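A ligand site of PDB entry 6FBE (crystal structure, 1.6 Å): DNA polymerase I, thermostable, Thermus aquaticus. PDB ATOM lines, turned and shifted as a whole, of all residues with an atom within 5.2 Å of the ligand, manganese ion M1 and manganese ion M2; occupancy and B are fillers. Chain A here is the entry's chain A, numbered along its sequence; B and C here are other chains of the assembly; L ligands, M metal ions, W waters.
The backbone NH (N) of Ile 323 lies close to an oxygen (O3) of the ligand, at 3.3 Å.
An oxygen (O8) of the ligand is in hydrogen-bond range of the backbone NH of Glu 324 (3.2 Å).
O4 of the ligand is in hydrogen-bond range of N of Gln 322 (3.0 Å).
The guanidinium group (NH1) of Arg 368 is in salt-bridge range of an oxygen (O7) of the ligand, 2.5 Å away.
O2 of DC 4 of chain C sits at hydrogen-bond distance from N2 of the ligand, at 2.7 Å.
A ring nitrogen (NE2) of His 348 is in hydrogen-bond range of an oxygen (O6) of the ligand, at 3.0 Å.
N3 of DG 5 of chain C lies close to N2 of the ligand, 3.3 Å away.
NH2 of Arg 282 lies within hydrogen-bond range of O11 of the ligand (3.1 Å).
The side-chain amino group of Lys 372 is in hydrogen-bond range of a nitrogen (N4) of the ligand (3.0 Å).
OH of Tyr 380 lies within hydrogen-bond range of OE1 of Glu 324 (2.7 Å).
O2 of DC 12 of chain B sits at hydrogen-bond distance from NH1 of Arg 282, 2.8 Å away.
The side-chain hydroxyl (OG) of Ser 321 lies within hydrogen-bond range of the side-chain amide nitrogen (NE2) of Gln 322 (3.3 Å).
The side-chain carboxylate (OD2) of Asp 319 lies close to the side-chain amino group (NZ) of Lys 540 (3.8 Å).
Ser 321 touches the ligand (CA to O4, 3.4 Å).
CZ of Phe 376 touches O8 of the ligand (3.1 Å).
Tyr 380 touches the ligand (CD2 to N2, 3.3 Å).
16 residues have an atom within 4 Å of the ligand: Arg 282, Asp 319, Tyr 320, Ser 321, Gln 322, Ile 323, Glu 324, His 348, Arg 368, Lys 372, Phe 376, Tyr 380, Asp 494, DC 12 of chain B, DC 4 of chain C and DG 5 of chain C.
The nearest printed residue that does not touch the ligand is Thr 373 (4.3 Å).
Within 4 Å of manganese ion M1: Asp 319, Asp 494 and DC 12 of chain B.
The nearest printed residue that does not touch manganese ion M1 is Glu 495 (4.2 Å).
The nearest printed residue that does not touch manganese ion M2 is Ser 321 (4.3 Å).
Manganese ion M1 is bound by the side-chain carboxylate (OD1) of Asp 494 (2.1 Å), the side-chain carboxylate (OD2) of Asp 319 (2.2 Å), water W10 (2.2 Å), water W9 (2.2 Å), O3' of DC 12 of chain B (2.2 Å) and an oxygen (O2) of the ligand (2.3 Å).
Manganese ion M1 has six donor atoms within binding distance.
Manganese ion M2 is bound by OD2 of Asp 494 (2.1 Å), O of Tyr 320 (2.1 Å), O10 of the ligand (2.1 Å), OD1 of Asp 319 (2.1 Å), O3 of the ligand (2.2 Å) and O2 of the ligand (2.3 Å).
Water W10 lies within hydrogen-bond range of the side-chain carboxylate of Glu 495 and the backbone carbonyl oxygen of Val 492.
Water W2 lies within hydrogen-bond range of the side-chain amino group of Lys 372, an oxygen (O5) of the ligand and OP2 of DC 12 of chain B.
Water W4 lies within hydrogen-bond range of the side-chain amino group of Lys 372 (2.8 Å), an oxygen (O1) of the ligand (2.8 Å), the side-chain hydroxyl of Thr 373 (2.8 Å) and N4 of DC 12 of chain B (3.4 Å).
Water W7 lies within hydrogen-bond range of OE2 of Glu 324 (2.8 Å), NH2 of Arg 282 (3.0 Å) and O11 of the ligand (3.5 Å).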
ATOM      1  N   ARG A 282      26.617 -16.069 -31.435  1.00  0.00           N
ATOM      2  CA  ARG A 282      26.944 -15.102 -30.393  1.00  0.00           C
ATOM      3  C   ARG A 282      27.306 -13.762 -31.015  1.00  0.00           C
ATOM      4  O   ARG A 282      27.760 -13.688 -32.172  1.00  0.00           O
ATOM      5  CB  ARG A 282      28.114 -15.587 -29.550  1.00  0.00           C
ATOM      6  CG  ARG A 282      27.758 -16.534 -28.437  1.00  0.00           C
ATOM      7  CD  ARG A 282      28.973 -16.726 -27.564  1.00  0.00           C
ATOM      8  NE  ARG A 282      28.680 -17.429 -26.325  1.00  0.00           N
ATOM      9  CZ  ARG A 282      29.576 -17.631 -25.365  1.00  0.00           C
ATOM     10  NH1 ARG A 282      30.809 -17.169 -25.505  1.00  0.00           N
ATOM     11  NH2 ARG A 282      29.233 -18.282 -24.266  1.00  0.00           N
ATOM     12  N   ASP A 319      21.887 -12.264 -15.179  1.00  0.00           N
ATOM     13  CA  ASP A 319      22.679 -13.341 -15.751  1.00  0.00           C
ATOM     14  C   ASP A 319      21.927 -14.664 -15.669  1.00  0.00           C
ATOM     15  O   ASP A 319      21.472 -15.040 -14.585  1.00  0.00           O
ATOM     16  CB  ASP A 319      24.034 -13.436 -15.039  1.00  0.00           C
ATOM     17  CG  ASP A 319      24.951 -14.443 -15.679  1.00  0.00           C
ATOM     18  OD1 ASP A 319      24.578 -15.630 -15.708  1.00  0.00           O
ATOM     19  OD2 ASP A 319      26.023 -14.041 -16.183  1.00  0.00           O
ATOM     20  N   TYR A 320      21.785 -15.344 -16.806  1.00  0.00           N
ATOM     21  CA  TYR A 320      21.078 -16.625 -16.827  1.00  0.00           C
ATOM     22  C   TYR A 320      21.850 -17.677 -16.028  1.00  0.00           C
ATOM     23  O   TYR A 320      23.068 -17.835 -16.181  1.00  0.00           O
ATOM     24  CB  TYR A 320      20.895 -17.127 -18.250  1.00  0.00           C
ATOM     25  CG  TYR A 320      19.780 -16.487 -19.058  1.00  0.00           C
ATOM     26  CD1 TYR A 320      18.443 -16.810 -18.833  1.00  0.00           C
ATOM     27  CD2 TYR A 320      20.075 -15.604 -20.091  1.00  0.00           C
ATOM     28  CE1 TYR A 320      17.439 -16.242 -19.591  1.00  0.00           C
ATOM     29  CE2 TYR A 320      19.071 -15.035 -20.848  1.00  0.00           C
ATOM     30  CZ  TYR A 320      17.760 -15.363 -20.599  1.00  0.00           C
ATOM     31  OH  TYR A 320      16.765 -14.799 -21.358  1.00  0.00           O
ATOM     32  N   SER A 321      21.115 -18.429 -15.208  1.00  0.00           N
ATOM     33  CA  SER A 321      21.697 -19.510 -14.421  1.00  0.00           C
ATOM     34  C   SER A 321      22.003 -20.723 -15.303  1.00  0.00           C
ATOM     35  O   SER A 321      21.113 -21.222 -15.999  1.00  0.00           O
ATOM     36  CB  SER A 321      20.737 -19.903 -13.289  1.00  0.00           C
ATOM     37  OG  SER A 321      21.106 -21.132 -12.691  1.00  0.00           O
ATOM     38  N   GLN A 322      23.242 -21.189 -15.262  1.00  0.00           N
ATOM     39  CA  GLN A 322      23.642 -22.478 -15.856  1.00  0.00           C
ATOM     40  C   GLN A 322      23.046 -22.659 -17.253  1.00  0.00           C
ATOM     41  O   GLN A 322      22.502 -23.707 -17.597  1.00  0.00           O
ATOM     42  CB  GLN A 322      23.209 -23.633 -14.965  1.00  0.00           C
ATOM     43  CG  GLN A 322      23.528 -23.463 -13.494  1.00  0.00           C
ATOM     44  CD  GLN A 322      22.946 -24.573 -12.649  1.00  0.00           C
ATOM     45  OE1 GLN A 322      23.374 -25.723 -12.734  1.00  0.00           O
ATOM     46  NE2 GLN A 322      21.950 -24.233 -11.839  1.00  0.00           N
ATOM     47  N   ILE A 323      23.169 -21.619 -18.087  1.00  0.00           N
ATOM     48  CA  ILE A 323      22.266 -21.524 -19.241  1.00  0.00           C
ATOM     49  C   ILE A 323      22.490 -22.678 -20.211  1.00  0.00           C
ATOM     50  O   ILE A 323      21.531 -23.297 -20.680  1.00  0.00           O
ATOM     51  CB  ILE A 323      22.391 -20.147 -19.922  1.00  0.00           C
ATOM     52  CG1 ILE A 323      21.369 -20.026 -21.055  1.00  0.00           C
ATOM     53  CG2 ILE A 323      23.794 -19.910 -20.471  1.00  0.00           C
ATOM     54  CD1 ILE A 323      19.917 -20.293 -20.656  1.00  0.00           C
ATOM     55  N   GLU A 324      23.749 -22.985 -20.546  1.00  0.00           N
ATOM     56  CA  GLU A 324      23.951 -23.999 -21.583  1.00  0.00           C
ATOM     57  C   GLU A 324      23.585 -25.383 -21.080  1.00  0.00           C
ATOM     58  O   GLU A 324      23.174 -26.243 -21.880  1.00  0.00           O
ATOM     59  CB  GLU A 324      25.381 -23.932 -22.126  1.00  0.00           C
ATOM     60  CG  GLU A 324      25.525 -22.824 -23.176  1.00  0.00           C
ATOM     61  CD  GLU A 324      26.854 -22.821 -23.912  1.00  0.00           C
ATOM     62  OE1 GLU A 324      27.553 -23.859 -23.925  1.00  0.00           O
ATOM     63  OE2 GLU A 324      27.209 -21.765 -24.471  1.00  0.00           O
ATOM     64  N   LEU A 325      23.681 -25.634 -19.779  1.00  0.00           N
ATOM     65  CA  LEU A 325      23.196 -26.909 -19.245  1.00  0.00           C
ATOM     66  C   LEU A 325      21.674 -26.985 -19.337  1.00  0.00           C
ATOM     67  O   LEU A 325      21.124 -28.062 -19.591  1.00  0.00           O
ATOM     68  CB  LEU A 325      23.668 -27.114 -17.810  1.00  0.00           C
ATOM     69  CG  LEU A 325      25.183 -27.200 -17.579  1.00  0.00           C
ATOM     70  CD1 LEU A 325      25.509 -27.395 -16.101  1.00  0.00           C
ATOM     71  CD2 LEU A 325      25.799 -28.333 -18.396  1.00  0.00           C
ATOM     72  N   HIS A 348      26.964 -26.619 -11.084  1.00  0.00           N
ATOM     73  CA  HIS A 348      28.273 -26.027 -10.833  1.00  0.00           C
ATOM     74  C   HIS A 348      28.651 -26.166  -9.357  1.00  0.00           C
ATOM     75  O   HIS A 348      29.763 -26.584  -9.022  1.00  0.00           O
ATOM     76  CB  HIS A 348      28.291 -24.552 -11.254  1.00  0.00           C
ATOM     77  CG  HIS A 348      28.098 -24.347 -12.720  1.00  0.00           C
ATOM     78  ND1 HIS A 348      28.470 -25.276 -13.660  1.00  0.00           N
ATOM     79  CD2 HIS A 348      27.577 -23.301 -13.414  1.00  0.00           C
ATOM     80  CE1 HIS A 348      28.180 -24.820 -14.869  1.00  0.00           C
ATOM     81  NE2 HIS A 348      27.633 -23.627 -14.745  1.00  0.00           N
ATOM     82  N   ARG A 368      33.236 -22.184  -7.536  1.00  0.00           N
ATOM     83  CA  ARG A 368      32.166 -22.403  -8.501  1.00  0.00           C
ATOM     84  C   ARG A 368      32.642 -22.084  -9.921  1.00  0.00           C
ATOM     85  O   ARG A 368      32.291 -22.785 -10.866  1.00  0.00           O
ATOM     86  CB  ARG A 368      30.939 -21.566  -8.123  1.00  0.00           C
ATOM     87  CG  ARG A 368      29.652 -22.052  -8.776  1.00  0.00           C
ATOM     88  CD  ARG A 368      28.417 -21.397  -8.170  1.00  0.00           C
ATOM     89  NE  ARG A 368      27.206 -21.733  -8.929  1.00  0.00           N
ATOM     90  CZ  ARG A 368      26.877 -21.176 -10.087  1.00  0.00           C
ATOM     91  NH1 ARG A 368      27.663 -20.246 -10.631  1.00  0.00           N
ATOM     92  NH2 ARG A 368      25.770 -21.545 -10.715  1.00  0.00           N
ATOM     93  N   LYS A 372      32.624 -24.578 -12.981  1.00  0.00           N
ATOM     94  CA  LYS A 372      32.003 -24.261 -14.261  1.00  0.00           C
ATOM     95  C   LYS A 372      32.881 -24.745 -15.415  1.00  0.00           C
ATOM     96  O   LYS A 372      32.407 -25.399 -16.352  1.00  0.00           O
ATOM     97  CB  LYS A 372      31.740 -22.761 -14.359  1.00  0.00           C
ATOM     98  CG  LYS A 372      31.165 -22.288 -15.695  1.00  0.00           C
ATOM     99  CD  LYS A 372      31.727 -20.929 -16.084  1.00  0.00           C
ATOM    100  CE  LYS A 372      33.176 -21.024 -16.526  1.00  0.00           C
ATOM    101  NZ  LYS A 372      33.664 -19.768 -17.163  1.00  0.00           N
ATOM    102  N   THR A 373      34.185 -24.438 -15.344  1.00  0.00           N
ATOM    103  CA  THR A 373      35.103 -24.844 -16.395  1.00  0.00           C
ATOM    104  C   THR A 373      35.146 -26.354 -16.535  1.00  0.00           C
ATOM    105  O   THR A 373      35.178 -26.884 -17.661  1.00  0.00           O
ATOM    106  CB  THR A 373      36.498 -24.287 -16.090  1.00  0.00           C
ATOM    107  OG1 THR A 373      36.409 -22.873 -15.881  1.00  0.00           O
ATOM    108  CG2 THR A 373      37.453 -24.557 -17.245  1.00  0.00           C
ATOM    109  N   PHE A 376      31.715 -27.690 -18.238  1.00  0.00           N
ATOM    110  CA  PHE A 376      31.630 -27.470 -19.675  1.00  0.00           C
ATOM    111  C   PHE A 376      32.802 -28.128 -20.398  1.00  0.00           C
ATOM    112  O   PHE A 376      32.616 -28.665 -21.500  1.00  0.00           O
ATOM    113  CB  PHE A 376      31.545 -25.981 -19.972  1.00  0.00           C
ATOM    114  CG  PHE A 376      30.252 -25.374 -19.511  1.00  0.00           C
ATOM    115  CD1 PHE A 376      29.051 -25.912 -19.918  1.00  0.00           C
ATOM    116  CD2 PHE A 376      30.244 -24.298 -18.626  1.00  0.00           C
ATOM    117  CE1 PHE A 376      27.854 -25.377 -19.476  1.00  0.00           C
ATOM    118  CE2 PHE A 376      29.052 -23.776 -18.183  1.00  0.00           C
ATOM    119  CZ  PHE A 376      27.858 -24.312 -18.614  1.00  0.00           C
ATOM    120  N   GLY A 377      33.981 -28.116 -19.795  1.00  0.00           N
ATOM    121  CA  GLY A 377      35.105 -28.839 -20.380  1.00  0.00           C
ATOM    122  C   GLY A 377      34.769 -30.298 -20.634  1.00  0.00           C
ATOM    123  O   GLY A 377      34.989 -30.813 -21.724  1.00  0.00           O
ATOM    124  N   TYR A 380      31.982 -30.842 -23.493  1.00  0.00           N
ATOM    125  CA  TYR A 380      32.338 -30.594 -24.877  1.00  0.00           C
ATOM    126  C   TYR A 380      33.604 -31.329 -25.313  1.00  0.00           C
ATOM    127  O   TYR A 380      34.210 -30.965 -26.314  1.00  0.00           O
ATOM    128  CB  TYR A 380      32.447 -29.089 -25.119  1.00  0.00           C
ATOM    129  CG  TYR A 380      31.105 -28.381 -24.952  1.00  0.00           C
ATOM    130  CD1 TYR A 380      30.014 -28.714 -25.747  1.00  0.00           C
ATOM    131  CD2 TYR A 380      30.919 -27.401 -23.969  1.00  0.00           C
ATOM    132  CE1 TYR A 380      28.792 -28.078 -25.596  1.00  0.00           C
ATOM    133  CE2 TYR A 380      29.689 -26.760 -23.815  1.00  0.00           C
ATOM    134  CZ  TYR A 380      28.634 -27.103 -24.631  1.00  0.00           C
ATOM    135  OH  TYR A 380      27.403 -26.478 -24.496  1.00  0.00           O
ATOM    136  N   ASN A 459      28.935 -28.544 -30.124  1.00  0.00           N
ATOM    137  CA  ASN A 459      28.854 -27.381 -29.250  1.00  0.00           C
ATOM    138  C   ASN A 459      27.894 -26.333 -29.803  1.00  0.00           C
ATOM    139  O   ASN A 459      27.158 -25.694 -29.039  1.00  0.00           O
ATOM    140  CB  ASN A 459      30.235 -26.758 -29.056  1.00  0.00           C
ATOM    141  CG  ASN A 459      30.189 -25.409 -28.355  1.00  0.00           C
ATOM    142  OD1 ASN A 459      30.070 -24.364 -29.001  1.00  0.00           O
ATOM    143  ND2 ASN A 459      30.263 -25.427 -27.027  1.00  0.00           N
ATOM    144  N   VAL A 492      26.825  -9.536 -22.231  1.00  0.00           N
ATOM    145  CA  VAL A 492      28.005 -10.394 -22.108  1.00  0.00           C
ATOM    146  C   VAL A 492      27.544 -11.840 -22.232  1.00  0.00           C
ATOM    147  O   VAL A 492      27.696 -12.639 -21.303  1.00  0.00           O
ATOM    148  CB  VAL A 492      28.751 -10.134 -20.788  1.00  0.00           C
ATOM    149  CG1 VAL A 492      30.124 -10.796 -20.823  1.00  0.00           C
ATOM    150  CG2 VAL A 492      28.913  -8.631 -20.540  1.00  0.00           C
ATOM    151  N   ASP A 494      25.324 -14.204 -21.870  1.00  0.00           N
ATOM    152  CA  ASP A 494      24.107 -14.589 -21.178  1.00  0.00           C
ATOM    153  C   ASP A 494      23.785 -13.599 -20.060  1.00  0.00           C
ATOM    154  O   ASP A 494      23.105 -13.952 -19.101  1.00  0.00           O
ATOM    155  CB  ASP A 494      24.218 -16.007 -20.624  1.00  0.00           C
ATOM    156  CG  ASP A 494      25.027 -16.071 -19.352  1.00  0.00           C
ATOM    157  OD1 ASP A 494      25.988 -15.282 -19.212  1.00  0.00           O
ATOM    158  OD2 ASP A 494      24.696 -16.921 -18.503  1.00  0.00           O
ATOM    159  N   GLU A 495      24.287 -12.379 -20.191  1.00  0.00           N
ATOM    160  CA  GLU A 495      24.177 -11.364 -19.161  1.00  0.00           C
ATOM    161  C   GLU A 495      23.835 -10.037 -19.812  1.00  0.00           C
ATOM    162  O   GLU A 495      24.317  -9.735 -20.914  1.00  0.00           O
ATOM    163  CB  GLU A 495      25.488 -11.247 -18.370  1.00  0.00           C
ATOM    164  CG  GLU A 495      25.564 -10.063 -17.409  1.00  0.00           C
ATOM    165  CD  GLU A 495      26.949  -9.891 -16.827  1.00  0.00           C
ATOM    166  OE1 GLU A 495      27.829 -10.725 -17.112  1.00  0.00           O
ATOM    167  OE2 GLU A 495      27.165  -8.921 -16.078  1.00  0.00           O
ATOM    168  N   LYS A 540      26.555  -7.489  -9.449  1.00  0.00           N
ATOM    169  CA  LYS A 540      26.548  -8.949  -9.570  1.00  0.00           C
ATOM    170  C   LYS A 540      26.590  -9.636  -8.213  1.00  0.00           C
ATOM    171  O   LYS A 540      27.056 -10.774  -8.110  1.00  0.00           O
ATOM    172  CB  LYS A 540      27.715  -9.419 -10.445  1.00  0.00           C
ATOM    173  CG  LYS A 540      27.774  -8.749 -11.819  1.00  0.00           C
ATOM    174  CD  LYS A 540      28.472  -9.635 -12.843  1.00  0.00           C
ATOM    175  CE  LYS A 540      27.537 -10.706 -13.383  1.00  0.00           C
ATOM    176  NZ  LYS A 540      28.252 -11.750 -14.168  1.00  0.00           N
ATOM    177  P    DC B  12      32.979 -13.683 -16.929  1.00  0.00           P
ATOM    178  OP1  DC B  12      32.022 -12.887 -16.131  1.00  0.00           O
ATOM    179  OP2  DC B  12      33.770 -14.757 -16.301  1.00  0.00           O
ATOM    180  O5'  DC B  12      32.218 -14.335 -18.169  1.00  0.00           O
ATOM    181  C5'  DC B  12      31.278 -13.564 -18.910  1.00  0.00           C
ATOM    182  C4'  DC B  12      30.702 -14.366 -20.059  1.00  0.00           C
ATOM    183  O4'  DC B  12      31.782 -14.791 -20.913  1.00  0.00           O
ATOM    184  C3'  DC B  12      29.995 -15.655 -19.657  1.00  0.00           C
ATOM    185  O3'  DC B  12      28.611 -15.410 -19.423  1.00  0.00           O
ATOM    186  C2'  DC B  12      30.212 -16.572 -20.848  1.00  0.00           C
ATOM    187  C1'  DC B  12      31.491 -16.044 -21.494  1.00  0.00           C
ATOM    188  N1   DC B  12      32.653 -16.937 -21.319  1.00  0.00           N
ATOM    189  C2   DC B  12      32.882 -17.945 -22.248  1.00  0.00           C
ATOM    190  O2   DC B  12      32.085 -18.075 -23.181  1.00  0.00           O
ATOM    191  N3   DC B  12      33.970 -18.723 -22.108  1.00  0.00           N
ATOM    192  C4   DC B  12      34.806 -18.538 -21.079  1.00  0.00           C
ATOM    193  N4   DC B  12      35.868 -19.349 -20.979  1.00  0.00           N
ATOM    194  C5   DC B  12      34.593 -17.516 -20.114  1.00  0.00           C
ATOM    195  C6   DC B  12      33.515 -16.735 -20.268  1.00  0.00           C
ATOM    196  P    DC C   4      41.441 -31.224 -24.487  1.00  0.00           P
ATOM    197  OP1  DC C   4      42.289 -30.069 -24.112  1.00  0.00           O
ATOM    198  OP2  DC C   4      41.558 -32.491 -23.746  1.00  0.00           O
ATOM    199  O5'  DC C   4      39.928 -30.721 -24.398  1.00  0.00           O
ATOM    200  C5'  DC C   4      39.535 -29.556 -25.105  1.00  0.00           C
ATOM    201  C4'  DC C   4      38.038 -29.507 -25.274  1.00  0.00           C
ATOM    202  O4'  DC C   4      37.409 -29.381 -23.976  1.00  0.00           O
ATOM    203  C3'  DC C   4      37.517 -28.323 -26.083  1.00  0.00           C
ATOM    204  O3'  DC C   4      37.518 -28.617 -27.474  1.00  0.00           O
ATOM    205  C2'  DC C   4      36.111 -28.148 -25.527  1.00  0.00           C
ATOM    206  C1'  DC C   4      36.298 -28.498 -24.060  1.00  0.00           C
ATOM    207  N1   DC C   4      36.558 -27.320 -23.185  1.00  0.00           N
ATOM    208  C2   DC C   4      35.531 -26.396 -22.943  1.00  0.00           C
ATOM    209  O2   DC C   4      34.428 -26.581 -23.471  1.00  0.00           O
ATOM    210  N3   DC C   4      35.769 -25.342 -22.139  1.00  0.00           N
ATOM    211  C4   DC C   4      36.977 -25.187 -21.585  1.00  0.00           C
ATOM    212  N4   DC C   4      37.171 -24.118 -20.802  1.00  0.00           N
ATOM    213  C5   DC C   4      38.040 -26.113 -21.818  1.00  0.00           C
ATOM    214  C6   DC C   4      37.789 -27.150 -22.620  1.00  0.00           C
ATOM    215  P    DG C   5      37.981 -27.504 -28.547  1.00  0.00           P
ATOM    216  OP1  DG C   5      38.222 -28.228 -29.825  1.00  0.00           O
ATOM    217  OP2  DG C   5      39.068 -26.693 -27.954  1.00  0.00           O
ATOM    218  O5'  DG C   5      36.702 -26.561 -28.695  1.00  0.00           O
ATOM    219  C5'  DG C   5      35.498 -27.073 -29.221  1.00  0.00           C
ATOM    220  C4'  DG C   5      34.350 -26.117 -28.978  1.00  0.00           C
ATOM    221  O4'  DG C   5      34.145 -25.959 -27.559  1.00  0.00           O
ATOM    222  C3'  DG C   5      34.568 -24.702 -29.492  1.00  0.00           C
ATOM    223  O3'  DG C   5      34.262 -24.594 -30.880  1.00  0.00           O
ATOM    224  C2'  DG C   5      33.621 -23.901 -28.614  1.00  0.00           C
ATOM    225  C1'  DG C   5      33.697 -24.645 -27.281  1.00  0.00           C
ATOM    226  N9   DG C   5      34.606 -24.025 -26.323  1.00  0.00           N
ATOM    227  C8   DG C   5      35.868 -24.457 -25.956  1.00  0.00           C
ATOM    228  N7   DG C   5      36.437 -23.689 -25.065  1.00  0.00           N
ATOM    229  C5   DG C   5      35.476 -22.704 -24.819  1.00  0.00           C
ATOM    230  C6   DG C   5      35.497 -21.588 -23.948  1.00  0.00           C
ATOM    231  O6   DG C   5      36.391 -21.227 -23.171  1.00  0.00           O
ATOM    232  N1   DG C   5      34.309 -20.851 -24.031  1.00  0.00           N
ATOM    233  C2   DG C   5      33.249 -21.158 -24.850  1.00  0.00           C
ATOM    234  N2   DG C   5      32.199 -20.346 -24.806  1.00  0.00           N
ATOM    235  N3   DG C   5      33.229 -22.190 -25.659  1.00  0.00           N
ATOM    236  C4   DG C   5      34.362 -22.909 -25.604  1.00  0.00           C
HETATM  237  N1  LIG L   1      33.702 -23.540 -21.801  1.00  0.00           N
HETATM  238  C1  LIG L   1      32.607 -23.605 -22.622  1.00  0.00           C
HETATM  239  N2  LIG L   1      32.592 -24.585 -23.524  1.00  0.00           N
HETATM  240  N3  LIG L   1      31.576 -22.770 -22.544  1.00  0.00           N
HETATM  241  C2  LIG L   1      31.707 -21.867 -21.561  1.00  0.00           C
HETATM  242  C3  LIG L   1      32.758 -21.710 -20.687  1.00  0.00           C
HETATM  243  C4  LIG L   1      33.868 -22.608 -20.779  1.00  0.00           C
HETATM  244  O1  LIG L   1      34.870 -22.632 -20.065  1.00  0.00           O
HETATM  245  N4  LIG L   1      32.505 -20.660 -19.809  1.00  0.00           N
HETATM  246  C5  LIG L   1      31.319 -20.223 -20.157  1.00  0.00           C
HETATM  247  N5  LIG L   1      30.771 -20.929 -21.200  1.00  0.00           N
HETATM  248  P1  LIG L   1      28.429 -18.178 -17.267  1.00  0.00           P
HETATM  249  P2  LIG L   1      26.649 -20.333 -16.360  1.00  0.00           P
HETATM  250  P3  LIG L   1      25.955 -19.322 -13.733  1.00  0.00           P
HETATM  251  C6  LIG L   1      29.397 -20.864 -21.724  1.00  0.00           C
HETATM  252  O2  LIG L   1      27.352 -17.199 -17.112  1.00  0.00           O
HETATM  253  O3  LIG L   1      25.601 -19.621 -17.083  1.00  0.00           O
HETATM  254  O4  LIG L   1      24.742 -19.930 -13.022  1.00  0.00           O
HETATM  255  C7  LIG L   1      28.484 -21.886 -21.066  1.00  0.00           C
HETATM  256  O5  LIG L   1      29.751 -17.541 -16.710  1.00  0.00           O
HETATM  257  O6  LIG L   1      26.766 -21.773 -16.943  1.00  0.00           O
HETATM  258  O7  LIG L   1      27.115 -19.066 -12.811  1.00  0.00           O
HETATM  259  C8  LIG L   1      27.821 -21.082 -19.957  1.00  0.00           C
HETATM  260  O8  LIG L   1      26.553 -21.648 -19.635  1.00  0.00           O
HETATM  261  N6  LIG L   1      28.093 -19.573 -16.509  1.00  0.00           N
HETATM  262  O9  LIG L   1      26.375 -20.434 -14.800  1.00  0.00           O
HETATM  263  O10 LIG L   1      25.560 -18.065 -14.559  1.00  0.00           O
HETATM  264  C9  LIG L   1      27.674 -19.725 -20.628  1.00  0.00           C
HETATM  265  O11 LIG L   1      28.870 -19.576 -21.429  1.00  0.00           O
HETATM  266  C10 LIG L   1      27.523 -18.547 -19.693  1.00  0.00           C
HETATM  267  O12 LIG L   1      28.645 -18.514 -18.781  1.00  0.00           O
HETATM  268 MN    MN M   1      27.363 -14.928 -17.620  1.00  0.00          MN
HETATM  269 MN    MN M   2      25.110 -17.511 -16.544  1.00  0.00          MN
HETATM  270  O   HOH W   1      29.675 -19.543 -13.818  1.00  0.00           O
HETATM  271  O   HOH W   2      32.468 -17.494 -16.709  1.00  0.00           O
HETATM  272  O   HOH W   3      27.504 -15.976 -13.789  1.00  0.00           O
HETATM  273  O   HOH W   4      35.986 -21.049 -18.029  1.00  0.00           O
HETATM  274  O   HOH W   5      30.011 -23.044 -25.102  1.00  0.00           O
HETATM  275  O   HOH W   6      23.612 -18.561 -11.009  1.00  0.00           O
HETATM  276  O   HOH W   7      26.382 -19.177 -23.824  1.00  0.00           O
HETATM  277  O   HOH W   8      23.497 -16.492 -13.073  1.00  0.00           O
HETATM  278  O   HOH W   9      29.049 -14.950 -16.175  1.00  0.00           O
HETATM  279  O   HOH W  10      28.095 -12.937 -18.106  1.00  0.00           O
